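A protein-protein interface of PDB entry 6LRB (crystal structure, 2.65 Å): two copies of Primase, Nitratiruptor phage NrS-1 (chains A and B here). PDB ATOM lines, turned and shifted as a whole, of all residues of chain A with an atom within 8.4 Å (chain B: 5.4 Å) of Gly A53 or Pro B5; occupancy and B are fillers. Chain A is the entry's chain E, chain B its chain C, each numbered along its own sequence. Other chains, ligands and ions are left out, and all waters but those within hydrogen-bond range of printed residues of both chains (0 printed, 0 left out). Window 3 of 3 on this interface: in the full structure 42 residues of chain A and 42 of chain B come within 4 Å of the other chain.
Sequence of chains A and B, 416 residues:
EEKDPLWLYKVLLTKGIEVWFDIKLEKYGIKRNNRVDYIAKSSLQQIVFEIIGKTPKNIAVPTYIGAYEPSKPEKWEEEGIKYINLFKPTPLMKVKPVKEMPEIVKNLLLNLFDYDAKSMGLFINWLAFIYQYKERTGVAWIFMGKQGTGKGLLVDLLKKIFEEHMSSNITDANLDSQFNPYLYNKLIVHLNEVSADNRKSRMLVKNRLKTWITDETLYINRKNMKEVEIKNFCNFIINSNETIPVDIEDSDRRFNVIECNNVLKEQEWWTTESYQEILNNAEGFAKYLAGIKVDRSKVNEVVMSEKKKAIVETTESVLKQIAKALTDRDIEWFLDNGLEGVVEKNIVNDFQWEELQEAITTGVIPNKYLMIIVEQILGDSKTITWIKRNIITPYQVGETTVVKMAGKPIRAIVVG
The backbone carbonyl oxygen of Ile B59 sits at hydrogen-bond distance from the side-chain amide nitrogen of Gln A46, at 3.0 Å.
The side-chain amide oxygen (OE1) of Gln A46 lies close to the backbone carbonyl oxygen (O) of Val B61 (3.4 Å).
Phe A49 touches Pro B5.
Phe A49 touches Ile B59 (CD2 to O, 3.6 Å).
CA of Ala B60 touches CE2 of Phe A49, 3.4 Å away.
Pro B5 touches Glu A50 (CB to O, 3.6 Å).
CG of Glu A50 touches O of Val B61 (3.7 Å).
Gly A53 touches Pro B5.
Printed residues of chain B within 4 Å of Gln A46: Ile B59 (3.0 Å) and Val B61 (3.4 Å).
Of the printed residues of chain B, Phe A49 touches Pro B5 (3.5 Å), Ile B59 (3.6 Å) and Ala B60 (3.4 Å).
Gly A53 touches just one residue of chain B: Pro B5 (3.9 Å).
Of chain A, only Phe A49 (3.5 Å), Glu A50 (3.6 Å) and Gly A53 (3.9 Å) come within 4 Å of Pro B5.
Of the printed residues of chain A, Ile B59 touches Gln A46 (3.0 Å) and Phe A49 (3.6 Å).
Of the printed residues of chain A, Ala B60 touches Phe A49 (3.4 Å).
Of the printed residues of chain A, Val B61 touches Gln A46 (3.4 Å) and Glu A50 (3.7 Å).
The nearest printed residue of chain B that does not touch Gly A53 is Asp B4 (5.9 Å).
Of the 14 printed residues of chain A, 4 touch a printed residue of chain B.
Printed residues of chain A that touch a printed residue of chain B: Gln A46, Phe A49, Glu A50 and Gly A53.
Hydrophobic or aromatic side chains of chain A within 4 Å of the printed part of chain B: Phe A49.
Printed residues of chain B that touch a printed residue of chain A: Pro B5, Ile B59, Ala B60 and Val B61.
Among the printed residues, 8 pairs touch across the chains.
Among the printed residues, no Asp or Glu carboxylate lies within 4 Å of a Lys or Arg side-chain nitrogen of the other chain.
No position is printed for both chains.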
ATOM      1  N   LEU A  12      23.972  28.388 -20.004  1.00  0.00           N
ATOM      2  CA  LEU A  12      24.486  28.928 -21.260  1.00  0.00           C
ATOM      3  C   LEU A  12      25.909  29.436 -21.087  1.00  0.00           C
ATOM      4  O   LEU A  12      26.678  29.345 -22.032  1.00  0.00           O
ATOM      5  CB  LEU A  12      23.567  30.007 -21.821  1.00  0.00           C
ATOM      6  CG  LEU A  12      22.151  29.539 -22.187  1.00  0.00           C
ATOM      7  CD1 LEU A  12      21.303  30.736 -22.576  1.00  0.00           C
ATOM      8  CD2 LEU A  12      22.101  28.496 -23.302  1.00  0.00           C
ATOM      9  N   LYS A  15      28.218  26.626 -21.633  1.00  0.00           N
ATOM     10  CA  LYS A  15      28.463  26.457 -23.058  1.00  0.00           C
ATOM     11  C   LYS A  15      29.117  27.660 -23.761  1.00  0.00           C
ATOM     12  O   LYS A  15      29.123  27.727 -24.991  1.00  0.00           O
ATOM     13  CB  LYS A  15      27.160  26.032 -23.751  1.00  0.00           C
ATOM     14  CG  LYS A  15      26.832  24.580 -23.457  1.00  0.00           C
ATOM     15  CD  LYS A  15      25.521  24.144 -24.077  1.00  0.00           C
ATOM     16  CE  LYS A  15      25.449  22.624 -24.193  1.00  0.00           C
ATOM     17  NZ  LYS A  15      25.576  21.933 -22.874  1.00  0.00           N
ATOM     18  N   GLN A  45      14.502  32.598 -27.372  1.00  0.00           N
ATOM     19  CA  GLN A  45      13.850  31.318 -27.127  1.00  0.00           C
ATOM     20  C   GLN A  45      14.249  30.284 -28.213  1.00  0.00           C
ATOM     21  O   GLN A  45      14.498  29.126 -27.906  1.00  0.00           O
ATOM     22  CB  GLN A  45      12.333  31.508 -27.088  1.00  0.00           C
ATOM     23  CG  GLN A  45      11.839  32.286 -25.880  1.00  0.00           C
ATOM     24  CD  GLN A  45      10.330  32.439 -25.864  1.00  0.00           C
ATOM     25  OE1 GLN A  45       9.724  32.915 -26.832  1.00  0.00           O
ATOM     26  NE2 GLN A  45       9.699  32.008 -24.769  1.00  0.00           N
ATOM     27  N   GLN A  46      14.350  30.724 -29.469  1.00  0.00           N
ATOM     28  CA  GLN A  46      14.793  29.847 -30.579  1.00  0.00           C
ATOM     29  C   GLN A  46      16.240  29.385 -30.428  1.00  0.00           C
ATOM     30  O   GLN A  46      16.554  28.240 -30.699  1.00  0.00           O
ATOM     31  CB  GLN A  46      14.601  30.559 -31.929  1.00  0.00           C
ATOM     32  CG  GLN A  46      15.096  29.821 -33.164  1.00  0.00           C
ATOM     33  CD  GLN A  46      14.694  28.365 -33.206  1.00  0.00           C
ATOM     34  OE1 GLN A  46      15.516  27.492 -33.518  1.00  0.00           O
ATOM     35  NE2 GLN A  46      13.424  28.087 -32.916  1.00  0.00           N
ATOM     36  N   ILE A  47      17.108  30.282 -30.000  1.00  0.00           N
ATOM     37  CA  ILE A  47      18.487  29.910 -29.687  1.00  0.00           C
ATOM     38  C   ILE A  47      18.556  28.952 -28.513  1.00  0.00           C
ATOM     39  O   ILE A  47      19.208  27.912 -28.591  1.00  0.00           O
ATOM     40  CB  ILE A  47      19.325  31.148 -29.333  1.00  0.00           C
ATOM     41  CG1 ILE A  47      19.617  31.899 -30.609  1.00  0.00           C
ATOM     42  CG2 ILE A  47      20.601  30.763 -28.588  1.00  0.00           C
ATOM     43  CD1 ILE A  47      20.437  33.141 -30.400  1.00  0.00           C
ATOM     44  N   VAL A  48      17.929  29.339 -27.414  1.00  0.00           N
ATOM     45  CA  VAL A  48      17.894  28.497 -26.218  1.00  0.00           C
ATOM     46  C   VAL A  48      17.418  27.086 -26.553  1.00  0.00           C
ATOM     47  O   VAL A  48      18.006  26.116 -26.105  1.00  0.00           O
ATOM     48  CB  VAL A  48      16.971  29.089 -25.126  1.00  0.00           C
ATOM     49  CG1 VAL A  48      16.726  28.094 -23.987  1.00  0.00           C
ATOM     50  CG2 VAL A  48      17.578  30.373 -24.564  1.00  0.00           C
ATOM     51  N   PHE A  49      16.351  26.969 -27.327  1.00  0.00           N
ATOM     52  CA  PHE A  49      15.843  25.645 -27.677  1.00  0.00           C
ATOM     53  C   PHE A  49      16.933  24.771 -28.286  1.00  0.00           C
ATOM     54  O   PHE A  49      17.157  23.642 -27.867  1.00  0.00           O
ATOM     55  CB  PHE A  49      14.668  25.732 -28.654  1.00  0.00           C
ATOM     56  CG  PHE A  49      14.140  24.381 -29.053  1.00  0.00           C
ATOM     57  CD1 PHE A  49      13.373  23.635 -28.170  1.00  0.00           C
ATOM     58  CD2 PHE A  49      14.435  23.832 -30.301  1.00  0.00           C
ATOM     59  CE1 PHE A  49      12.885  22.380 -28.530  1.00  0.00           C
ATOM     60  CE2 PHE A  49      13.963  22.576 -30.648  1.00  0.00           C
ATOM     61  CZ  PHE A  49      13.185  21.850 -29.769  1.00  0.00           C
ATOM     62  N   GLU A  50      17.583  25.315 -29.298  1.00  0.00           N
ATOM     63  CA  GLU A  50      18.651  24.623 -30.035  1.00  0.00           C
ATOM     64  C   GLU A  50      19.761  24.108 -29.122  1.00  0.00           C
ATOM     65  O   GLU A  50      20.387  23.101 -29.440  1.00  0.00           O
ATOM     66  CB  GLU A  50      19.232  25.597 -31.065  1.00  0.00           C
ATOM     67  CG  GLU A  50      20.316  25.049 -31.973  1.00  0.00           C
ATOM     68  CD  GLU A  50      21.303  26.106 -32.424  1.00  0.00           C
ATOM     69  OE1 GLU A  50      21.391  27.199 -31.818  1.00  0.00           O
ATOM     70  OE2 GLU A  50      21.993  25.844 -33.430  1.00  0.00           O
ATOM     71  N   ILE A  51      19.986  24.793 -27.996  1.00  0.00           N
ATOM     72  CA  ILE A  51      21.134  24.534 -27.103  1.00  0.00           C
ATOM     73  C   ILE A  51      20.820  23.649 -25.897  1.00  0.00           C
ATOM     74  O   ILE A  51      21.699  22.953 -25.426  1.00  0.00           O
ATOM     75  CB  ILE A  51      21.780  25.876 -26.658  1.00  0.00           C
ATOM     76  CG1 ILE A  51      22.335  26.614 -27.896  1.00  0.00           C
ATOM     77  CG2 ILE A  51      22.912  25.666 -25.651  1.00  0.00           C
ATOM     78  CD1 ILE A  51      22.821  28.023 -27.649  1.00  0.00           C
ATOM     79  N   ILE A  52      19.596  23.695 -25.376  1.00  0.00           N
ATOM     80  CA  ILE A  52      19.189  22.805 -24.258  1.00  0.00           C
ATOM     81  C   ILE A  52      18.045  21.841 -24.581  1.00  0.00           C
ATOM     82  O   ILE A  52      17.747  20.954 -23.782  1.00  0.00           O
ATOM     83  CB  ILE A  52      18.879  23.601 -22.954  1.00  0.00           C
ATOM     84  CG1 ILE A  52      17.601  24.450 -23.069  1.00  0.00           C
ATOM     85  CG2 ILE A  52      20.079  24.471 -22.577  1.00  0.00           C
ATOM     86  CD1 ILE A  52      17.260  25.263 -21.826  1.00  0.00           C
ATOM     87  N   GLY A  53      17.376  22.031 -25.718  1.00  0.00           N
ATOM     88  CA  GLY A  53      16.232  21.183 -26.118  1.00  0.00           C
ATOM     89  C   GLY A  53      14.904  21.469 -25.440  1.00  0.00           C
ATOM     90  O   GLY A  53      13.986  20.654 -25.508  1.00  0.00           O
ATOM     91  N   LYS A  54      14.806  22.615 -24.772  1.00  0.00           N
ATOM     92  CA  LYS A  54      13.641  22.995 -23.980  1.00  0.00           C
ATOM     93  C   LYS A  54      13.405  24.477 -24.228  1.00  0.00           C
ATOM     94  O   LYS A  54      14.341  25.271 -24.161  1.00  0.00           O
ATOM     95  CB  LYS A  54      13.887  22.743 -22.470  1.00  0.00           C
ATOM     96  N   THR A  55      12.156  24.832 -24.524  1.00  0.00           N
ATOM     97  CA  THR A  55      11.735  26.222 -24.639  1.00  0.00           C
ATOM     98  C   THR A  55      11.045  26.569 -23.331  1.00  0.00           C
ATOM     99  O   THR A  55       9.893  26.132 -23.107  1.00  0.00           O
ATOM    100  CB  THR A  55      10.774  26.420 -25.827  1.00  0.00           C
ATOM    101  OG1 THR A  55      11.359  25.862 -27.010  1.00  0.00           O
ATOM    102  CG2 THR A  55      10.514  27.890 -26.073  1.00  0.00           C
ATOM    103  N   PRO A  56      11.741  27.307 -22.437  1.00  0.00           N
ATOM    104  CA  PRO A  56      11.088  27.711 -21.188  1.00  0.00           C
ATOM    105  C   PRO A  56      10.199  28.920 -21.442  1.00  0.00           C
ATOM    106  O   PRO A  56      10.514  29.727 -22.320  1.00  0.00           O
ATOM    107  CB  PRO A  56      12.267  28.106 -20.297  1.00  0.00           C
ATOM    108  CG  PRO A  56      13.265  28.656 -21.261  1.00  0.00           C
ATOM    109  CD  PRO A  56      13.075  27.917 -22.559  1.00  0.00           C
ATOM    110  N   LYS B   3      13.973  14.681 -26.850  1.00  0.00           N
ATOM    111  CA  LYS B   3      15.156  13.843 -27.239  1.00  0.00           C
ATOM    112  C   LYS B   3      16.172  14.640 -28.093  1.00  0.00           C
ATOM    113  O   LYS B   3      17.366  14.699 -27.757  1.00  0.00           O
ATOM    114  CB  LYS B   3      14.680  12.585 -27.970  1.00  0.00           C
ATOM    115  N   ASP B   4      15.688  15.262 -29.176  1.00  0.00           N
ATOM    116  CA  ASP B   4      16.548  15.865 -30.207  1.00  0.00           C
ATOM    117  C   ASP B   4      16.206  17.333 -30.526  1.00  0.00           C
ATOM    118  O   ASP B   4      15.118  17.614 -30.992  1.00  0.00           O
ATOM    119  CB  ASP B   4      16.428  15.037 -31.485  1.00  0.00           C
ATOM    120  CG  ASP B   4      17.476  15.392 -32.513  1.00  0.00           C
ATOM    121  OD1 ASP B   4      18.338  16.249 -32.244  1.00  0.00           O
ATOM    122  OD2 ASP B   4      17.460  14.776 -33.605  1.00  0.00           O
ATOM    123  N   PRO B   5      17.142  18.271 -30.287  1.00  0.00           N
ATOM    124  CA  PRO B   5      16.944  19.688 -30.689  1.00  0.00           C
ATOM    125  C   PRO B   5      16.925  20.046 -32.198  1.00  0.00           C
ATOM    126  O   PRO B   5      16.600  21.186 -32.535  1.00  0.00           O
ATOM    127  CB  PRO B   5      18.128  20.404 -30.022  1.00  0.00           C
ATOM    128  CG  PRO B   5      18.499  19.530 -28.868  1.00  0.00           C
ATOM    129  CD  PRO B   5      18.287  18.130 -29.365  1.00  0.00           C
ATOM    130  N   LEU B   6      17.295  19.108 -33.075  1.00  0.00           N
ATOM    131  CA  LEU B   6      17.360  19.344 -34.522  1.00  0.00           C
ATOM    132  C   LEU B   6      16.559  18.352 -35.343  1.00  0.00           C
ATOM    133  O   LEU B   6      16.759  18.263 -36.546  1.00  0.00           O
ATOM    134  CB  LEU B   6      18.818  19.295 -34.977  1.00  0.00           C
ATOM    135  CG  LEU B   6      19.840  20.179 -34.249  1.00  0.00           C
ATOM    136  CD1 LEU B   6      21.222  19.940 -34.844  1.00  0.00           C
ATOM    137  CD2 LEU B   6      19.497  21.661 -34.325  1.00  0.00           C
ATOM    138  N   TRP B   7      15.636  17.607 -34.731  1.00  0.00           N
ATOM    139  CA  TRP B   7      14.901  16.579 -35.471  1.00  0.00           C
ATOM    140  C   TRP B   7      14.292  17.169 -36.748  1.00  0.00           C
ATOM    141  O   TRP B   7      14.489  16.632 -37.841  1.00  0.00           O
ATOM    142  CB  TRP B   7      13.841  15.879 -34.605  1.00  0.00           C
ATOM    143  CG  TRP B   7      12.698  16.743 -34.205  1.00  0.00           C
ATOM    144  CD1 TRP B   7      12.604  17.543 -33.100  1.00  0.00           C
ATOM    145  CD2 TRP B   7      11.470  16.900 -34.915  1.00  0.00           C
ATOM    146  NE1 TRP B   7      11.388  18.196 -33.075  1.00  0.00           N
ATOM    147  CE2 TRP B   7      10.673  17.821 -34.184  1.00  0.00           C
ATOM    148  CE3 TRP B   7      10.968  16.365 -36.109  1.00  0.00           C
ATOM    149  CZ2 TRP B   7       9.400  18.205 -34.610  1.00  0.00           C
ATOM    150  CZ3 TRP B   7       9.693  16.743 -36.518  1.00  0.00           C
ATOM    151  CH2 TRP B   7       8.927  17.658 -35.774  1.00  0.00           C
ATOM    152  N   ILE B  59      10.521  25.167 -33.028  1.00  0.00           N
ATOM    153  CA  ILE B  59      11.159  24.979 -34.305  1.00  0.00           C
ATOM    154  C   ILE B  59      12.550  24.407 -34.029  1.00  0.00           C
ATOM    155  O   ILE B  59      13.430  25.107 -33.516  1.00  0.00           O
ATOM    156  CB  ILE B  59      11.262  26.298 -35.112  1.00  0.00           C
ATOM    157  CG1 ILE B  59       9.906  27.035 -35.172  1.00  0.00           C
ATOM    158  CG2 ILE B  59      11.755  26.015 -36.526  1.00  0.00           C
ATOM    159  CD1 ILE B  59       8.744  26.196 -35.659  1.00  0.00           C
ATOM    160  N   ALA B  60      12.705  23.118 -34.346  1.00  0.00           N
ATOM    161  CA  ALA B  60      13.874  22.341 -33.989  1.00  0.00           C
ATOM    162  C   ALA B  60      14.844  22.415 -35.105  1.00  0.00           C
ATOM    163  O   ALA B  60      14.940  21.496 -35.892  1.00  0.00           O
ATOM    164  CB  ALA B  60      13.481  20.894 -33.680  1.00  0.00           C
ATOM    165  N   VAL B  61      15.555  23.536 -35.171  1.00  0.00           N
ATOM    166  CA  VAL B  61      16.505  23.814 -36.244  1.00  0.00           C
ATOM    167  C   VAL B  61      17.758  24.508 -35.711  1.00  0.00           C
ATOM    168  O   VAL B  61      17.721  25.122 -34.645  1.00  0.00           O
ATOM    169  CB  VAL B  61      15.882  24.709 -37.352  1.00  0.00           C
ATOM    170  CG1 VAL B  61      14.681  24.034 -37.992  1.00  0.00           C
ATOM    171  CG2 VAL B  61      15.498  26.079 -36.811  1.00  0.00           C
